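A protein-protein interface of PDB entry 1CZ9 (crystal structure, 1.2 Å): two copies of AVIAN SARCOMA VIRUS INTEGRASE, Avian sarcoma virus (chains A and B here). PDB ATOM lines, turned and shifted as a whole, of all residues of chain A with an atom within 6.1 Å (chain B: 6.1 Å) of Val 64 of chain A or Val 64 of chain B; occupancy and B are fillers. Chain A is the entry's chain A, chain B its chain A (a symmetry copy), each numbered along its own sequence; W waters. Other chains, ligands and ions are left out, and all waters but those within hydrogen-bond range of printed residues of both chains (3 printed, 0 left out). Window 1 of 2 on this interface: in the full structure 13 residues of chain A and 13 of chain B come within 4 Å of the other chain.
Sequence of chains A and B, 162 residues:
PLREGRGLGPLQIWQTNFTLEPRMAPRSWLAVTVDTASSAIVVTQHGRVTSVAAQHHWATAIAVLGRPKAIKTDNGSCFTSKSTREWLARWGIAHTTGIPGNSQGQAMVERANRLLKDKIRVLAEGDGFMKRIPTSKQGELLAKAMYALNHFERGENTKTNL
Water W3 lies within hydrogen-bond range of O of Ala 63 of chain A (2.6 Å) and O of Met 146 of chain B (3.4 Å). Water W1 lies within hydrogen-bond range of the backbone carbonyl oxygen of Ala 63 of chain B (2.6 Å) and the backbone carbonyl oxygen of Met 146 of chain A (3.4 Å). Water W2 lies within hydrogen-bond range of the backbone carbonyl oxygen (O) of Val 64 of chain A and the backbone carbonyl oxygen (O) of Val 64 of chain B.
Of the 11 printed residues of chain A, 3 touch a printed residue of chain B. Hydrophobic or aromatic side chains of chain A that line the printed part of chain B: Val 64 and Met 146. Printed residues of chain B that touch a printed residue of chain A: Ala 63, Val 64 and Met 146. Hydrophobic or aromatic side chains of chain B within 4 Å of the printed part of chain A: Val 64 and Met 146. Among the printed residues, no Asp or Glu carboxylate lies within 4 Å of a Lys or Arg side-chain nitrogen of the other chain.
Met 146 of chain B touches Ala 63 of chain A. Val 64 of chain A touches Val 64 of chain B (CG2 to CG2, 3.9 Å). Met 146 of chain A touches Ala 63 of chain B.
Ala 63 of chain A touches Met 146 of chain B, and with the chains exchanged Met 146 of chain A touches Ala 63 of chain B. Val 64 of chain B touches its own counterpart, Val 64 of chain A.
Of chain B, only Val 64 comes within 4 Å of Val 64 of chain A. Of the printed residues of chain B, Met 146 of chain A touches Ala 63 (3.5 Å). Ala 59 of chain B touches none of the printed residues of chain A. Of the printed residues of chain A, Met 146 of chain B touches Ala 63. The nearest residue of chain B that does not touch Val 64 of chain A is Ala 63 of chain B (4.7 Å). The nearest printed residue of chain B that does not touch Met 146 of chain A is Val 64 of chain B (5.0 Å).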
ATOM      1  N   ILE A  41      18.315 -28.985  -6.192  1.00  0.00           N
ATOM      2  CA  ILE A  41      18.725 -28.010  -7.214  1.00  0.00           C
ATOM      3  C   ILE A  41      19.117 -26.683  -6.568  1.00  0.00           C
ATOM      4  O   ILE A  41      18.513 -26.245  -5.552  1.00  0.00           O
ATOM      5  CB  ILE A  41      17.518 -27.842  -8.158  1.00  0.00           C
ATOM      6  CG1 ILE A  41      17.266 -29.125  -8.968  1.00  0.00           C
ATOM      7  CG2 ILE A  41      17.532 -26.655  -9.058  1.00  0.00           C
ATOM      8  CD1 ILE A  41      15.845 -29.232  -9.560  1.00  0.00           C
ATOM      9  N   VAL A  42      20.120 -26.041  -7.164  1.00  0.00           N
ATOM     10  CA  VAL A  42      20.458 -24.647  -6.911  1.00  0.00           C
ATOM     11  C   VAL A  42      20.394 -23.914  -8.237  1.00  0.00           C
ATOM     12  O   VAL A  42      20.931 -24.394  -9.226  1.00  0.00           O
ATOM     13  CB  VAL A  42      21.838 -24.471  -6.286  1.00  0.00           C
ATOM     14  CG1 VAL A  42      22.176 -23.014  -6.104  1.00  0.00           C
ATOM     15  CG2 VAL A  42      21.886 -25.207  -4.940  1.00  0.00           C
ATOM     16  N   ALA A  59      29.814 -20.774  -6.093  1.00  0.00           N
ATOM     17  CA  ALA A  59      30.037 -20.223  -4.767  1.00  0.00           C
ATOM     18  C   ALA A  59      28.730 -20.235  -3.986  1.00  0.00           C
ATOM     19  O   ALA A  59      28.679 -20.609  -2.792  1.00  0.00           O
ATOM     20  CB  ALA A  59      30.601 -18.811  -4.873  1.00  0.00           C
ATOM     21  N   THR A  60      27.656 -19.815  -4.638  1.00  0.00           N
ATOM     22  CA  THR A  60      26.338 -19.869  -4.031  1.00  0.00           C
ATOM     23  C   THR A  60      25.939 -21.309  -3.715  1.00  0.00           C
ATOM     24  O   THR A  60      25.449 -21.605  -2.613  1.00  0.00           O
ATOM     25  CB  THR A  60      25.301 -19.190  -4.924  1.00  0.00           C
ATOM     26  OG1 THR A  60      25.621 -17.800  -5.019  1.00  0.00           O
ATOM     27  CG2 THR A  60      23.898 -19.334  -4.379  1.00  0.00           C
ATOM     28  N   ALA A  61      26.119 -22.212  -4.673  1.00  0.00           N
ATOM     29  CA  ALA A  61      25.733 -23.589  -4.507  1.00  0.00           C
ATOM     30  C   ALA A  61      26.483 -24.203  -3.344  1.00  0.00           C
ATOM     31  O   ALA A  61      25.859 -25.020  -2.624  1.00  0.00           O
ATOM     32  CB  ALA A  61      25.904 -24.369  -5.796  1.00  0.00           C
ATOM     33  N   ILE A  62      27.760 -23.901  -3.162  1.00  0.00           N
ATOM     34  CA  ILE A  62      28.510 -24.453  -2.019  1.00  0.00           C
ATOM     35  C   ILE A  62      27.925 -23.982  -0.722  1.00  0.00           C
ATOM     36  O   ILE A  62      27.842 -24.749   0.248  1.00  0.00           O
ATOM     37  CB  ILE A  62      30.008 -24.069  -2.171  1.00  0.00           C
ATOM     38  CG1 ILE A  62      30.645 -24.821  -3.343  1.00  0.00           C
ATOM     39  CG2 ILE A  62      30.787 -24.325  -0.883  1.00  0.00           C
ATOM     40  CD1 ILE A  62      32.035 -24.311  -3.717  1.00  0.00           C
ATOM     41  N   ALA A  63      27.513 -22.699  -0.637  1.00  0.00           N
ATOM     42  CA  ALA A  63      26.878 -22.153   0.548  1.00  0.00           C
ATOM     43  C   ALA A  63      25.517 -22.830   0.827  1.00  0.00           C
ATOM     44  O   ALA A  63      25.080 -22.872   1.981  1.00  0.00           O
ATOM     45  CB  ALA A  63      26.680 -20.666   0.409  1.00  0.00           C
ATOM     46  N   VAL A  64      24.844 -23.358  -0.163  1.00  0.00           N
ATOM     47  CA  VAL A  64      23.562 -24.015  -0.007  1.00  0.00           C
ATOM     48  C   VAL A  64      23.715 -25.509   0.286  1.00  0.00           C
ATOM     49  O   VAL A  64      23.015 -25.979   1.211  1.00  0.00           O
ATOM     50  CB  VAL A  64      22.671 -23.811  -1.255  1.00  0.00           C
ATOM     51  CG1 VAL A  64      21.364 -24.616  -1.113  1.00  0.00           C
ATOM     52  CG2 VAL A  64      22.377 -22.366  -1.505  1.00  0.00           C
ATOM     53  N   LEU A  65      24.572 -26.220  -0.443  1.00  0.00           N
ATOM     54  CA  LEU A  65      24.631 -27.663  -0.423  1.00  0.00           C
ATOM     55  C   LEU A  65      25.863 -28.271   0.269  1.00  0.00           C
ATOM     56  O   LEU A  65      25.903 -29.450   0.581  1.00  0.00           O
ATOM     57  CB  LEU A  65      24.667 -28.143  -1.877  1.00  0.00           C
ATOM     58  CG  LEU A  65      23.449 -27.857  -2.742  1.00  0.00           C
ATOM     59  CD1 LEU A  65      23.607 -28.412  -4.145  1.00  0.00           C
ATOM     60  CD2 LEU A  65      22.182 -28.413  -2.100  1.00  0.00           C
ATOM     61  N   GLY A  66      26.891 -27.465   0.435  1.00  0.00           N
ATOM     62  CA  GLY A  66      28.197 -27.913   0.866  1.00  0.00           C
ATOM     63  C   GLY A  66      29.146 -28.033  -0.303  1.00  0.00           C
ATOM     64  O   GLY A  66      28.779 -27.849  -1.461  1.00  0.00           O
ATOM     65  N   MET A 146      12.774 -22.735  -6.660  1.00  0.00           N
ATOM     66  CA  MET A 146      13.799 -23.608  -6.066  1.00  0.00           C
ATOM     67  C   MET A 146      13.276 -24.312  -4.828  1.00  0.00           C
ATOM     68  O   MET A 146      13.423 -25.540  -4.659  1.00  0.00           O
ATOM     69  CB  MET A 146      15.053 -22.775  -5.794  1.00  0.00           C
ATOM     70  CG  MET A 146      16.179 -23.545  -5.168  1.00  0.00           C
ATOM     71  SD  MET A 146      17.642 -22.504  -5.057  1.00  0.00           S
ATOM     72  CE  MET A 146      18.544 -23.347  -3.741  1.00  0.00           C
ATOM     73  N   ILE B  41      23.228 -20.839   9.369  1.00  0.00           N
ATOM     74  CA  ILE B  41      23.041 -19.413   9.063  1.00  0.00           C
ATOM     75  C   ILE B  41      22.791 -19.208   7.572  1.00  0.00           C
ATOM     76  O   ILE B  41      23.370 -19.920   6.706  1.00  0.00           O
ATOM     77  CB  ILE B  41      24.330 -18.702   9.522  1.00  0.00           C
ATOM     78  CG1 ILE B  41      24.461 -18.725  11.054  1.00  0.00           C
ATOM     79  CG2 ILE B  41      24.554 -17.323   9.003  1.00  0.00           C
ATOM     80  CD1 ILE B  41      25.894 -18.484  11.572  1.00  0.00           C
ATOM     81  N   VAL B  42      21.939 -18.230   7.271  1.00  0.00           N
ATOM     82  CA  VAL B  42      21.782 -17.668   5.937  1.00  0.00           C
ATOM     83  C   VAL B  42      22.053 -16.179   6.035  1.00  0.00           C
ATOM     84  O   VAL B  42      21.532 -15.521   6.925  1.00  0.00           O
ATOM     85  CB  VAL B  42      20.397 -17.907   5.347  1.00  0.00           C
ATOM     86  CG1 VAL B  42      20.254 -17.251   3.997  1.00  0.00           C
ATOM     87  CG2 VAL B  42      20.140 -19.416   5.242  1.00  0.00           C
ATOM     88  N   ALA B  59      13.033 -15.013   1.511  1.00  0.00           N
ATOM     89  CA  ALA B  59      12.787 -15.809   0.321  1.00  0.00           C
ATOM     90  C   ALA B  59      14.014 -16.657   0.015  1.00  0.00           C
ATOM     91  O   ALA B  59      13.918 -17.864  -0.305  1.00  0.00           O
ATOM     92  CB  ALA B  59      12.438 -14.904  -0.855  1.00  0.00           C
ATOM     93  N   THR B  60      15.184 -16.042   0.093  1.00  0.00           N
ATOM     94  CA  THR B  60      16.429 -16.766  -0.082  1.00  0.00           C
ATOM     95  C   THR B  60      16.595 -17.841   0.991  1.00  0.00           C
ATOM     96  O   THR B  60      16.951 -18.991   0.689  1.00  0.00           O
ATOM     97  CB  THR B  60      17.619 -15.807  -0.095  1.00  0.00           C
ATOM     98  OG1 THR B  60      17.507 -14.957  -1.238  1.00  0.00           O
ATOM     99  CG2 THR B  60      18.940 -16.539  -0.156  1.00  0.00           C
ATOM    100  N   ALA B  61      16.365 -17.480   2.249  1.00  0.00           N
ATOM    101  CA  ALA B  61      16.538 -18.393   3.349  1.00  0.00           C
ATOM    102  C   ALA B  61      15.620 -19.586   3.184  1.00  0.00           C
ATOM    103  O   ALA B  61      16.064 -20.706   3.535  1.00  0.00           O
ATOM    104  CB  ALA B  61      16.359 -17.691   4.681  1.00  0.00           C
ATOM    105  N   ILE B  62      14.389 -19.401   2.733  1.00  0.00           N
ATOM    106  CA  ILE B  62      13.482 -20.544   2.528  1.00  0.00           C
ATOM    107  C   ILE B  62      14.023 -21.473   1.484  1.00  0.00           C
ATOM    108  O   ILE B  62      13.922 -22.701   1.616  1.00  0.00           O
ATOM    109  CB  ILE B  62      12.069 -20.004   2.169  1.00  0.00           C
ATOM    110  CG1 ILE B  62      11.425 -19.321   3.379  1.00  0.00           C
ATOM    111  CG2 ILE B  62      11.164 -21.111   1.635  1.00  0.00           C
ATOM    112  CD1 ILE B  62      10.156 -18.544   3.041  1.00  0.00           C
ATOM    113  N   ALA B  63      14.605 -20.932   0.391  1.00  0.00           N
ATOM    114  CA  ALA B  63      15.217 -21.734  -0.653  1.00  0.00           C
ATOM    115  C   ALA B  63      16.442 -22.514  -0.126  1.00  0.00           C
ATOM    116  O   ALA B  63      16.777 -23.569  -0.674  1.00  0.00           O
ATOM    117  CB  ALA B  63      15.633 -20.870  -1.814  1.00  0.00           C
ATOM    118  N   VAL B  64      17.109 -22.052   0.901  1.00  0.00           N
ATOM    119  CA  VAL B  64      18.269 -22.707   1.469  1.00  0.00           C
ATOM    120  C   VAL B  64      17.884 -23.712   2.558  1.00  0.00           C
ATOM    121  O   VAL B  64      18.436 -24.834   2.513  1.00  0.00           O
ATOM    122  CB  VAL B  64      19.274 -21.677   2.035  1.00  0.00           C
ATOM    123  CG1 VAL B  64      20.440 -22.402   2.738  1.00  0.00           C
ATOM    124  CG2 VAL B  64      19.789 -20.755   0.976  1.00  0.00           C
ATOM    125  N   LEU B  65      16.995 -23.349   3.479  1.00  0.00           N
ATOM    126  CA  LEU B  65      16.732 -24.111   4.677  1.00  0.00           C
ATOM    127  C   LEU B  65      15.376 -24.835   4.722  1.00  0.00           C
ATOM    128  O   LEU B  65      15.145 -25.707   5.545  1.00  0.00           O
ATOM    129  CB  LEU B  65      16.742 -23.132   5.856  1.00  0.00           C
ATOM    130  CG  LEU B  65      18.051 -22.428   6.173  1.00  0.00           C
ATOM    131  CD1 LEU B  65      17.927 -21.515   7.379  1.00  0.00           C
ATOM    132  CD2 LEU B  65      19.173 -23.437   6.397  1.00  0.00           C
ATOM    133  N   GLY B  66      14.462 -24.409   3.875  1.00  0.00           N
ATOM    134  CA  GLY B  66      13.076 -24.821   3.920  1.00  0.00           C
ATOM    135  C   GLY B  66      12.214 -23.767   4.572  1.00  0.00           C
ATOM    136  O   GLY B  66      12.692 -22.748   5.065  1.00  0.00           O
ATOM    137  N   MET B 146      29.616 -17.967   4.794  1.00  0.00           N
ATOM    138  CA  MET B 146      28.435 -18.778   5.131  1.00  0.00           C
ATOM    139  C   MET B 146      28.755 -20.260   5.102  1.00  0.00           C
ATOM    140  O   MET B 146      28.424 -21.022   6.033  1.00  0.00           O
ATOM    141  CB  MET B 146      27.294 -18.395   4.186  1.00  0.00           C
ATOM    142  CG  MET B 146      26.024 -19.164   4.412  1.00  0.00           C
ATOM    143  SD  MET B 146      24.720 -18.507   3.363  1.00  0.00           S
ATOM    144  CE  MET B 146      23.607 -19.927   3.297  1.00  0.00           C
HETATM  145  O   HOH W   1      15.187 -25.292  -1.760  1.00  0.00           O
HETATM  146  O   HOH W   2      20.645 -26.275   2.342  1.00  0.00           O
HETATM  147  O   HOH W   3      26.491 -23.082   4.135  1.00  0.00           O
